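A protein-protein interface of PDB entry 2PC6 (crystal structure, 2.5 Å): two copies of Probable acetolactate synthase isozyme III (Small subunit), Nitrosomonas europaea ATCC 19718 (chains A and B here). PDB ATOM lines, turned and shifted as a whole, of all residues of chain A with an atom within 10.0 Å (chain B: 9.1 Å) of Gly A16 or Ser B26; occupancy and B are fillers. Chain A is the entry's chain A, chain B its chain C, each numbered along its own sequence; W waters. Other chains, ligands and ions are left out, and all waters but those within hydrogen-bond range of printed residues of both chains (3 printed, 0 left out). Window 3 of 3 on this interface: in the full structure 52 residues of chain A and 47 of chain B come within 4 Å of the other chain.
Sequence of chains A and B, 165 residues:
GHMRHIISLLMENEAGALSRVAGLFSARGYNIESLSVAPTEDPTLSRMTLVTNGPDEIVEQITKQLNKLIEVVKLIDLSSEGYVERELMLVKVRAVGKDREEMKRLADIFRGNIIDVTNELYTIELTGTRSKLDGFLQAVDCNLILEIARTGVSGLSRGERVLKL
OD1 of Asn A13 sits at hydrogen-bond distance from ND2 of Asn B31. OD1 of Asn B31 lies close to O of Glu A14 (3.5 Å). O of Ser A19 sits at hydrogen-bond distance from OG of Ser B19. The backbone NH (N) of Gly A23 is in hydrogen-bond range of the side-chain hydroxyl (OG) of Ser B19, at 3.5 Å. The backbone NH (N) of Ala A15 is in hydrogen-bond range of the side-chain amide oxygen (OD1) of Asn B31, at 3.5 Å.
O of Ala B22 sits at hydrogen-bond distance from OG of Ser B26, 2.4 Å away. The side-chain hydroxyl (OG) of Ser A19 lies within hydrogen-bond range of the backbone carbonyl oxygen (O) of Gly A16 (2.9 Å). O of Gly B23 lies close to OG of Ser B26 (3.5 Å). O of Asn B31 is in hydrogen-bond range of OG1 of Thr B52. The backbone carbonyl oxygen (O) of Ala A15 sits at hydrogen-bond distance from the guanidinium group (NH2) of Arg A20, 3.1 Å away.
OG of Ser B26 touches CA of Gly A16 (3.8 Å). Leu A18 touches Leu B18 (CD2 to CD2, 3.97 Å). CB of Ser A19 touches CB of Ala B22 (3.8 Å). Gly B23 touches Ser A19 (N to CB, 3.8 Å). CB of Ser A19 touches OG of Ser B26, 3.8 Å away. Leu B18 touches Ala A22 (CD2 to CB, 3.96 Å). CB of Ser B19 touches CB of Ala A22, 3.5 Å away.
Water W1 lies within hydrogen-bond range of the side-chain hydroxyl (OG) of Ser B26, the backbone NH (N) of Ser A19 and the backbone carbonyl oxygen (O) of Ala B22. Water W3 bridges the backbone carbonyl oxygen (O) of Ser B26 (2.9 Å) and the backbone carbonyl oxygen (O) of Ala A15 (3.2 Å). Water W2 lies within hydrogen-bond range of the side-chain amide oxygen of Asn A13 (3.0 Å) and the backbone carbonyl oxygen of Ile B32 (3.4 Å).
Ser A19 touches its own counterpart, Ser B19. Ser A19 touches Ala B22, and with the chains exchanged Ala A22 touches Ser B19. Ser A19 touches Gly B23, and with the chains exchanged Gly A23 touches Ser B19. Ala A22 touches Leu B18, but with the chains exchanged Leu A18 does not touch Ala B22 (4.1 Å). Positions printed for both chains: 18, 19, 20, 21, 22, 23 and 24. Of the 12 pairs that touch across the chains among the printed residues, 6 have their exchanged pair printed and touching as well.
Hydrophobic or aromatic side chains of chain B within 4 Å of the printed part of chain A: Leu B18 and Ala B22. Hydrophobic or aromatic side chains of chain A that line the printed part of chain B: Leu A18 and Ala A22. Among the printed residues, 12 pairs touch across the chains. Among the printed residues, no Asp or Glu carboxylate lies within 4 Å of a Lys or Arg side-chain nitrogen of the other chain.
Ala A15 touches one residue of chain B. No residue of chain B comes within 4 Å of Ala A17. Gly B23 touches just one residue of chain A: Ser A19 (3.8 Å). Of the printed residues of chain B, Ala A22 touches Leu B18 and Ser B19. Of the printed residues of chain A, Leu B18 touches Leu A18 (3.97 Å) and Ala A22 (3.96 Å). Of the printed residues of chain A, Ser B19 touches Ser A19, Ala A22 and Gly A23. Val A72 touches none of the printed residues of chain B. The nearest residue of chain A that does not touch Ser B26 is Ala A15 (4.5 Å). The nearest printed residue of chain B that does not touch Asn A13 is Ile B32 (4.1 Å).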
ATOM      1  N   MET A  11      -9.205  26.433  10.988  1.00  0.00           N
ATOM      2  CA  MET A  11      -9.213  27.497  10.015  1.00  0.00           C
ATOM      3  C   MET A  11     -10.537  27.823   9.412  1.00  0.00           C
ATOM      4  O   MET A  11     -11.439  26.989   9.372  1.00  0.00           O
ATOM      5  CB  MET A  11      -8.196  27.249   8.922  1.00  0.00           C
ATOM      6  CG  MET A  11      -8.077  25.844   8.441  1.00  0.00           C
ATOM      7  SD  MET A  11      -7.481  26.139   6.636  1.00  0.00           S
ATOM      8  CE  MET A  11      -9.161  25.563   5.535  1.00  0.00           C
ATOM      9  N   GLU A  12     -10.633  29.074   8.968  1.00  0.00           N
ATOM     10  CA  GLU A  12     -11.748  29.580   8.178  1.00  0.00           C
ATOM     11  C   GLU A  12     -12.118  28.621   7.052  1.00  0.00           C
ATOM     12  O   GLU A  12     -11.326  28.393   6.132  1.00  0.00           O
ATOM     13  CB  GLU A  12     -11.402  30.955   7.588  1.00  0.00           C
ATOM     14  CG  GLU A  12     -10.938  32.052   8.601  1.00  0.00           C
ATOM     15  CD  GLU A  12     -12.005  32.495   9.642  1.00  0.00           C
ATOM     16  OE1 GLU A  12     -13.077  31.852   9.809  1.00  0.00           O
ATOM     17  OE2 GLU A  12     -11.754  33.513  10.312  1.00  0.00           O
ATOM     18  N   ASN A  13     -13.316  28.045   7.135  1.00  0.00           N
ATOM     19  CA  ASN A  13     -13.817  27.182   6.080  1.00  0.00           C
ATOM     20  C   ASN A  13     -14.223  28.002   4.839  1.00  0.00           C
ATOM     21  O   ASN A  13     -15.425  28.171   4.501  1.00  0.00           O
ATOM     22  CB  ASN A  13     -14.952  26.311   6.600  1.00  0.00           C
ATOM     23  CG  ASN A  13     -15.433  25.310   5.572  1.00  0.00           C
ATOM     24  OD1 ASN A  13     -14.738  24.987   4.587  1.00  0.00           O
ATOM     25  ND2 ASN A  13     -16.632  24.828   5.780  1.00  0.00           N
ATOM     26  N   GLU A  14     -13.210  28.526   4.162  1.00  0.00           N
ATOM     27  CA  GLU A  14     -13.457  29.417   3.021  1.00  0.00           C
ATOM     28  C   GLU A  14     -12.515  29.118   1.847  1.00  0.00           C
ATOM     29  O   GLU A  14     -11.508  28.410   2.004  1.00  0.00           O
ATOM     30  CB  GLU A  14     -13.404  30.902   3.435  1.00  0.00           C
ATOM     31  CG  GLU A  14     -12.044  31.335   3.949  1.00  0.00           C
ATOM     32  CD  GLU A  14     -11.984  32.783   4.416  1.00  0.00           C
ATOM     33  OE1 GLU A  14     -13.039  33.392   4.684  1.00  0.00           O
ATOM     34  OE2 GLU A  14     -10.864  33.321   4.523  1.00  0.00           O
ATOM     35  N   ALA A  15     -12.869  29.680   0.689  1.00  0.00           N
ATOM     36  CA  ALA A  15     -12.211  29.401  -0.596  1.00  0.00           C
ATOM     37  C   ALA A  15     -10.817  30.017  -0.602  1.00  0.00           C
ATOM     38  O   ALA A  15     -10.654  31.230  -0.418  1.00  0.00           O
ATOM     39  CB  ALA A  15     -13.059  29.970  -1.793  1.00  0.00           C
ATOM     40  N   GLY A  16      -9.817  29.169  -0.818  1.00  0.00           N
ATOM     41  CA  GLY A  16      -8.442  29.629  -0.891  1.00  0.00           C
ATOM     42  C   GLY A  16      -7.696  29.343   0.396  1.00  0.00           C
ATOM     43  O   GLY A  16      -6.476  29.159   0.381  1.00  0.00           O
ATOM     44  N   ALA A  17      -8.440  29.301   1.500  1.00  0.00           N
ATOM     45  CA  ALA A  17      -7.881  28.938   2.819  1.00  0.00           C
ATOM     46  C   ALA A  17      -6.844  27.856   2.680  1.00  0.00           C
ATOM     47  O   ALA A  17      -5.703  28.007   3.144  1.00  0.00           O
ATOM     48  CB  ALA A  17      -8.967  28.448   3.748  1.00  0.00           C
ATOM     49  N   LEU A  18      -7.230  26.764   2.029  1.00  0.00           N
ATOM     50  CA  LEU A  18      -6.341  25.613   1.967  1.00  0.00           C
ATOM     51  C   LEU A  18      -5.254  25.832   0.923  1.00  0.00           C
ATOM     52  O   LEU A  18      -4.096  25.403   1.136  1.00  0.00           O
ATOM     53  CB  LEU A  18      -7.094  24.280   1.714  1.00  0.00           C
ATOM     54  CG  LEU A  18      -6.121  23.178   1.234  1.00  0.00           C
ATOM     55  CD1 LEU A  18      -5.233  22.690   2.389  1.00  0.00           C
ATOM     56  CD2 LEU A  18      -6.822  21.997   0.594  1.00  0.00           C
ATOM     57  N   SER A  19      -5.590  26.463  -0.206  1.00  0.00           N
ATOM     58  CA  SER A  19      -4.537  26.714  -1.192  1.00  0.00           C
ATOM     59  C   SER A  19      -3.438  27.640  -0.618  1.00  0.00           C
ATOM     60  O   SER A  19      -2.268  27.516  -0.986  1.00  0.00           O
ATOM     61  CB  SER A  19      -5.083  27.305  -2.499  1.00  0.00           C
ATOM     62  OG  SER A  19      -5.367  28.667  -2.261  1.00  0.00           O
ATOM     63  N   ARG A  20      -3.818  28.554   0.281  1.00  0.00           N
ATOM     64  CA  ARG A  20      -2.831  29.411   0.936  1.00  0.00           C
ATOM     65  C   ARG A  20      -1.964  28.659   1.969  1.00  0.00           C
ATOM     66  O   ARG A  20      -0.761  28.915   2.083  1.00  0.00           O
ATOM     67  CB  ARG A  20      -3.492  30.658   1.535  1.00  0.00           C
ATOM     68  CG  ARG A  20      -3.749  31.700   0.453  1.00  0.00           C
ATOM     69  CD  ARG A  20      -4.430  33.002   0.972  1.00  0.00           C
ATOM     70  NE  ARG A  20      -5.859  32.811   1.211  1.00  0.00           N
ATOM     71  CZ  ARG A  20      -6.790  32.906   0.256  1.00  0.00           C
ATOM     72  NH1 ARG A  20      -6.439  33.166  -1.007  1.00  0.00           N
ATOM     73  NH2 ARG A  20      -8.080  32.726   0.557  1.00  0.00           N
ATOM     74  N   VAL A  21      -2.571  27.739   2.718  1.00  0.00           N
ATOM     75  CA  VAL A  21      -1.827  26.926   3.634  1.00  0.00           C
ATOM     76  C   VAL A  21      -0.878  26.003   2.852  1.00  0.00           C
ATOM     77  O   VAL A  21       0.282  25.832   3.232  1.00  0.00           O
ATOM     78  CB  VAL A  21      -2.759  26.164   4.576  1.00  0.00           C
ATOM     79  CG1 VAL A  21      -2.014  25.000   5.282  1.00  0.00           C
ATOM     80  CG2 VAL A  21      -3.327  27.158   5.596  1.00  0.00           C
ATOM     81  N   ALA A  22      -1.332  25.457   1.724  1.00  0.00           N
ATOM     82  CA  ALA A  22      -0.459  24.557   0.952  1.00  0.00           C
ATOM     83  C   ALA A  22       0.604  25.355   0.239  1.00  0.00           C
ATOM     84  O   ALA A  22       1.731  24.847   0.059  1.00  0.00           O
ATOM     85  CB  ALA A  22      -1.247  23.698  -0.014  1.00  0.00           C
ATOM     86  N   GLY A  23       0.288  26.605  -0.131  1.00  0.00           N
ATOM     87  CA  GLY A  23       1.264  27.445  -0.804  1.00  0.00           C
ATOM     88  C   GLY A  23       2.456  27.796   0.086  1.00  0.00           C
ATOM     89  O   GLY A  23       3.619  27.776  -0.337  1.00  0.00           O
ATOM     90  N   LEU A  24       2.166  28.118   1.335  1.00  0.00           N
ATOM     91  CA  LEU A  24       3.196  28.407   2.334  1.00  0.00           C
ATOM     92  C   LEU A  24       4.246  27.260   2.434  1.00  0.00           C
ATOM     93  O   LEU A  24       5.437  27.529   2.396  1.00  0.00           O
ATOM     94  CB  LEU A  24       2.518  28.702   3.679  1.00  0.00           C
ATOM     95  CG  LEU A  24       3.347  29.049   4.915  1.00  0.00           C
ATOM     96  CD1 LEU A  24       2.473  29.758   5.943  1.00  0.00           C
ATOM     97  CD2 LEU A  24       3.950  27.788   5.520  1.00  0.00           C
ATOM     98  N   MET A  48      -7.854  21.006  10.537  1.00  0.00           N
ATOM     99  CA  MET A  48      -6.898  20.384   9.675  1.00  0.00           C
ATOM    100  C   MET A  48      -5.920  19.638  10.516  1.00  0.00           C
ATOM    101  O   MET A  48      -5.449  20.141  11.541  1.00  0.00           O
ATOM    102  CB  MET A  48      -6.169  21.419   8.849  1.00  0.00           C
ATOM    103  CG  MET A  48      -5.126  20.830   7.928  1.00  0.00           C
ATOM    104  SD  MET A  48      -4.318  22.242   6.778  1.00  0.00           S
ATOM    105  CE  MET A  48      -5.983  22.937   5.892  1.00  0.00           C
ATOM    106  N   LEU A  69      -0.733  33.525   9.179  1.00  0.00           N
ATOM    107  CA  LEU A  69      -1.854  33.547   8.239  1.00  0.00           C
ATOM    108  C   LEU A  69      -3.101  33.939   8.995  1.00  0.00           C
ATOM    109  O   LEU A  69      -3.337  33.405  10.057  1.00  0.00           O
ATOM    110  CB  LEU A  69      -2.067  32.172   7.598  1.00  0.00           C
ATOM    111  CG  LEU A  69      -0.941  31.551   6.773  1.00  0.00           C
ATOM    112  CD1 LEU A  69      -1.343  30.210   6.209  1.00  0.00           C
ATOM    113  CD2 LEU A  69      -0.486  32.496   5.634  1.00  0.00           C
ATOM    114  N   GLU A  71      -6.160  33.207   8.255  1.00  0.00           N
ATOM    115  CA  GLU A  71      -7.180  32.161   8.154  1.00  0.00           C
ATOM    116  C   GLU A  71      -6.912  30.986   9.112  1.00  0.00           C
ATOM    117  O   GLU A  71      -7.782  30.125   9.322  1.00  0.00           O
ATOM    118  CB  GLU A  71      -7.343  31.682   6.708  1.00  0.00           C
ATOM    119  CG  GLU A  71      -8.102  32.660   5.799  1.00  0.00           C
ATOM    120  CD  GLU A  71      -7.893  32.359   4.312  1.00  0.00           C
ATOM    121  OE1 GLU A  71      -6.845  31.794   3.929  1.00  0.00           O
ATOM    122  OE2 GLU A  71      -8.778  32.711   3.514  1.00  0.00           O
ATOM    123  N   VAL A  72      -5.707  30.968   9.684  1.00  0.00           N
ATOM    124  CA  VAL A  72      -5.347  30.028  10.708  1.00  0.00           C
ATOM    125  C   VAL A  72      -5.638  30.641  12.087  1.00  0.00           C
ATOM    126  O   VAL A  72      -5.074  31.651  12.465  1.00  0.00           O
ATOM    127  CB  VAL A  72      -3.882  29.698  10.564  1.00  0.00           C
ATOM    128  CG1 VAL A  72      -3.342  28.994  11.839  1.00  0.00           C
ATOM    129  CG2 VAL A  72      -3.666  28.848   9.265  1.00  0.00           C
ATOM    130  N   LEU B  18      -0.517  20.122  -4.481  1.00  0.00           N
ATOM    131  CA  LEU B  18      -1.682  20.381  -3.643  1.00  0.00           C
ATOM    132  C   LEU B  18      -2.222  21.789  -3.870  1.00  0.00           C
ATOM    133  O   LEU B  18      -3.320  21.965  -4.396  1.00  0.00           O
ATOM    134  CB  LEU B  18      -1.335  20.182  -2.166  1.00  0.00           C
ATOM    135  CG  LEU B  18      -2.395  19.487  -1.308  1.00  0.00           C
ATOM    136  CD1 LEU B  18      -1.748  18.761  -0.139  1.00  0.00           C
ATOM    137  CD2 LEU B  18      -3.430  20.488  -0.817  1.00  0.00           C
ATOM    138  N   SER B  19      -1.443  22.788  -3.468  1.00  0.00           N
ATOM    139  CA  SER B  19      -1.891  24.207  -3.541  1.00  0.00           C
ATOM    140  C   SER B  19      -2.431  24.577  -4.919  1.00  0.00           C
ATOM    141  O   SER B  19      -3.367  25.382  -5.040  1.00  0.00           O
ATOM    142  CB  SER B  19      -0.739  25.178  -3.191  1.00  0.00           C
ATOM    143  OG  SER B  19      -1.142  26.531  -3.288  1.00  0.00           O
ATOM    144  N   ARG B  20      -1.812  23.978  -5.940  1.00  0.00           N
ATOM    145  CA  ARG B  20      -2.152  24.254  -7.334  1.00  0.00           C
ATOM    146  C   ARG B  20      -3.506  23.621  -7.671  1.00  0.00           C
ATOM    147  O   ARG B  20      -4.314  24.241  -8.350  1.00  0.00           O
ATOM    148  CB  ARG B  20      -1.047  23.770  -8.304  1.00  0.00           C
ATOM    149  CG  ARG B  20      -1.100  24.451  -9.667  1.00  0.00           C
ATOM    150  CD  ARG B  20       0.212  24.423 -10.412  1.00  0.00           C
ATOM    151  NE  ARG B  20      -0.032  24.927 -11.767  1.00  0.00           N
ATOM    152  CZ  ARG B  20       0.722  24.657 -12.834  1.00  0.00           C
ATOM    153  NH1 ARG B  20       1.801  23.891 -12.719  1.00  0.00           N
ATOM    154  NH2 ARG B  20       0.402  25.149 -14.026  1.00  0.00           N
ATOM    155  N   VAL B  21      -3.764  22.411  -7.152  1.00  0.00           N
ATOM    156  CA  VAL B  21      -5.069  21.784  -7.338  1.00  0.00           C
ATOM    157  C   VAL B  21      -6.135  22.548  -6.547  1.00  0.00           C
ATOM    158  O   VAL B  21      -7.217  22.851  -7.051  1.00  0.00           O
ATOM    159  CB  VAL B  21      -5.060  20.280  -6.945  1.00  0.00           C
ATOM    160  CG1 VAL B  21      -6.483  19.758  -6.850  1.00  0.00           C
ATOM    161  CG2 VAL B  21      -4.227  19.459  -7.978  1.00  0.00           C
ATOM    162  N   ALA B  22      -5.794  22.864  -5.306  1.00  0.00           N
ATOM    163  CA  ALA B  22      -6.678  23.556  -4.421  1.00  0.00           C
ATOM    164  C   ALA B  22      -7.010  24.903  -5.042  1.00  0.00           C
ATOM    165  O   ALA B  22      -8.148  25.363  -4.938  1.00  0.00           O
ATOM    166  CB  ALA B  22      -6.016  23.716  -3.070  1.00  0.00           C
ATOM    167  N   GLY B  23      -6.017  25.488  -5.729  1.00  0.00           N
ATOM    168  CA  GLY B  23      -6.118  26.800  -6.346  1.00  0.00           C
ATOM    169  C   GLY B  23      -7.187  26.898  -7.412  1.00  0.00           C
ATOM    170  O   GLY B  23      -7.955  27.847  -7.454  1.00  0.00           O
ATOM    171  N   LEU B  24      -7.263  25.881  -8.257  1.00  0.00           N
ATOM    172  CA  LEU B  24      -8.219  25.866  -9.374  1.00  0.00           C
ATOM    173  C   LEU B  24      -9.714  25.866  -8.954  1.00  0.00           C
ATOM    174  O   LEU B  24     -10.549  26.429  -9.671  1.00  0.00           O
ATOM    175  CB  LEU B  24      -7.883  24.708 -10.335  1.00  0.00           C
ATOM    176  CG  LEU B  24      -6.503  24.797 -11.040  1.00  0.00           C
ATOM    177  CD1 LEU B  24      -6.196  23.562 -11.931  1.00  0.00           C
ATOM    178  CD2 LEU B  24      -6.301  26.100 -11.818  1.00  0.00           C
ATOM    179  N   PHE B  25     -10.036  25.266  -7.802  1.00  0.00           N
ATOM    180  CA  PHE B  25     -11.356  25.463  -7.150  1.00  0.00           C
ATOM    181  C   PHE B  25     -11.472  26.855  -6.519  1.00  0.00           C
ATOM    182  O   PHE B  25     -12.429  27.596  -6.794  1.00  0.00           O
ATOM    183  CB  PHE B  25     -11.650  24.355  -6.121  1.00  0.00           C
ATOM    184  CG  PHE B  25     -11.621  22.977  -6.705  1.00  0.00           C
ATOM    185  CD1 PHE B  25     -10.486  22.173  -6.562  1.00  0.00           C
ATOM    186  CD2 PHE B  25     -12.710  22.494  -7.446  1.00  0.00           C
ATOM    187  CE1 PHE B  25     -10.434  20.904  -7.136  1.00  0.00           C
ATOM    188  CE2 PHE B  25     -12.679  21.205  -8.041  1.00  0.00           C
ATOM    189  CZ  PHE B  25     -11.539  20.405  -7.889  1.00  0.00           C
ATOM    190  N   SER B  26     -10.482  27.221  -5.707  1.00  0.00           N
ATOM    191  CA  SER B  26     -10.362  28.596  -5.205  1.00  0.00           C
ATOM    192  C   SER B  26     -10.493  29.600  -6.342  1.00  0.00           C
ATOM    193  O   SER B  26     -11.229  30.578  -6.229  1.00  0.00           O
ATOM    194  CB  SER B  26      -8.999  28.794  -4.555  1.00  0.00           C
ATOM    195  OG  SER B  26      -8.533  27.560  -4.035  1.00  0.00           O
ATOM    196  N   ALA B  27      -9.781  29.335  -7.440  1.00  0.00           N
ATOM    197  CA  ALA B  27      -9.739  30.218  -8.616  1.00  0.00           C
ATOM    198  C   ALA B  27     -11.151  30.623  -9.051  1.00  0.00           C
ATOM    199  O   ALA B  27     -11.404  31.794  -9.340  1.00  0.00           O
ATOM    200  N   ARG B  28     -12.075  29.655  -9.042  1.00  0.00           N
ATOM    201  CA  ARG B  28     -13.443  29.897  -9.515  1.00  0.00           C
ATOM    202  C   ARG B  28     -14.365  30.408  -8.380  1.00  0.00           C
ATOM    203  O   ARG B  28     -15.554  30.635  -8.587  1.00  0.00           O
ATOM    204  CB  ARG B  28     -13.979  28.616 -10.170  1.00  0.00           C
ATOM    205  CG  ARG B  28     -14.486  28.809 -11.595  1.00  0.00           C
ATOM    206  CD  ARG B  28     -13.376  28.823 -12.646  1.00  0.00           C
ATOM    207  NE  ARG B  28     -13.773  29.640 -13.812  1.00  0.00           N
ATOM    208  N   GLY B  29     -13.786  30.601  -7.189  1.00  0.00           N
ATOM    209  CA  GLY B  29     -14.532  30.929  -5.964  1.00  0.00           C
ATOM    210  C   GLY B  29     -15.278  29.755  -5.318  1.00  0.00           C
ATOM    211  O   GLY B  29     -16.281  29.971  -4.622  1.00  0.00           O
ATOM    212  N   TYR B  30     -14.805  28.522  -5.537  1.00  0.00           N
ATOM    213  CA  TYR B  30     -15.504  27.339  -5.007  1.00  0.00           C
ATOM    214  C   TYR B  30     -14.825  26.709  -3.814  1.00  0.00           C
ATOM    215  O   TYR B  30     -13.638  26.413  -3.855  1.00  0.00           O
ATOM    216  CB  TYR B  30     -15.835  26.274  -6.087  1.00  0.00           C
ATOM    217  CG  TYR B  30     -17.067  26.667  -6.883  1.00  0.00           C
ATOM    218  CD1 TYR B  30     -17.242  26.282  -8.217  1.00  0.00           C
ATOM    219  CD2 TYR B  30     -18.044  27.504  -6.298  1.00  0.00           C
ATOM    220  CE1 TYR B  30     -18.385  26.699  -8.927  1.00  0.00           C
ATOM    221  CE2 TYR B  30     -19.165  27.921  -6.985  1.00  0.00           C
ATOM    222  CZ  TYR B  30     -19.345  27.523  -8.295  1.00  0.00           C
ATOM    223  OH  TYR B  30     -20.499  27.970  -8.944  1.00  0.00           O
ATOM    224  N   ASN B  31     -15.603  26.504  -2.756  1.00  0.00           N
ATOM    225  CA  ASN B  31     -15.110  25.896  -1.516  1.00  0.00           C
ATOM    226  C   ASN B  31     -14.867  24.385  -1.566  1.00  0.00           C
ATOM    227  O   ASN B  31     -15.761  23.629  -1.935  1.00  0.00           O
ATOM    228  CB  ASN B  31     -16.059  26.201  -0.343  1.00  0.00           C
ATOM    229  CG  ASN B  31     -15.394  25.981   1.006  1.00  0.00           C
ATOM    230  OD1 ASN B  31     -14.369  26.600   1.298  1.00  0.00           O
ATOM    231  ND2 ASN B  31     -15.955  25.094   1.821  1.00  0.00           N
ATOM    232  N   ILE B  32     -13.670  23.959  -1.167  1.00  0.00           N
ATOM    233  CA  ILE B  32     -13.380  22.543  -0.916  1.00  0.00           C
ATOM    234  C   ILE B  32     -13.931  22.206   0.476  1.00  0.00           C
ATOM    235  O   ILE B  32     -13.419  22.690   1.484  1.00  0.00           O
ATOM    236  CB  ILE B  32     -11.839  22.219  -1.012  1.00  0.00           C
ATOM    237  CG1 ILE B  32     -11.248  22.669  -2.356  1.00  0.00           C
ATOM    238  CG2 ILE B  32     -11.513  20.679  -0.764  1.00  0.00           C
ATOM    239  N   LEU B  50     -11.355  14.562  -2.946  1.00  0.00           N
ATOM    240  CA  LEU B  50     -11.809  15.920  -2.667  1.00  0.00           C
ATOM    241  C   LEU B  50     -13.269  16.042  -2.983  1.00  0.00           C
ATOM    242  O   LEU B  50     -13.681  15.759  -4.116  1.00  0.00           O
ATOM    243  CB  LEU B  50     -11.018  16.901  -3.536  1.00  0.00           C
ATOM    244  CG  LEU B  50     -11.372  18.373  -3.649  1.00  0.00           C
ATOM    245  CD1 LEU B  50     -10.071  19.098  -4.058  1.00  0.00           C
ATOM    246  CD2 LEU B  50     -12.472  18.638  -4.683  1.00  0.00           C
ATOM    247  N   THR B  52     -16.667  18.438  -3.252  1.00  0.00           N
ATOM    248  CA  THR B  52     -16.901  19.858  -3.574  1.00  0.00           C
ATOM    249  C   THR B  52     -18.326  20.071  -4.055  1.00  0.00           C
ATOM    250  O   THR B  52     -19.060  19.092  -4.237  1.00  0.00           O
ATOM    251  CB  THR B  52     -15.862  20.419  -4.640  1.00  0.00           C
ATOM    252  OG1 THR B  52     -15.962  21.850  -4.725  1.00  0.00           O
ATOM    253  CG2 THR B  52     -16.085  19.826  -6.042  1.00  0.00           C
ATOM    254  N   ILE B  62     -12.789  22.574 -14.314  1.00  0.00           N
ATOM    255  CA  ILE B  62     -11.641  22.361 -13.438  1.00  0.00           C
ATOM    256  C   ILE B  62     -10.918  21.054 -13.778  1.00  0.00           C
ATOM    257  O   ILE B  62      -9.710  21.053 -14.012  1.00  0.00           O
ATOM    258  CB  ILE B  62     -12.047  22.390 -11.954  1.00  0.00           C
ATOM    259  CG1 ILE B  62     -12.992  23.566 -11.683  1.00  0.00           C
ATOM    260  CG2 ILE B  62     -10.813  22.499 -11.075  1.00  0.00           C
HETATM  261  O   HOH W   1      -8.120  26.200  -1.595  1.00  0.00           O
HETATM  262  O   HOH W   2     -13.431  22.336   4.817  1.00  0.00           O
HETATM  263  O   HOH W   3     -11.017  31.662  -3.595  1.00  0.00           O
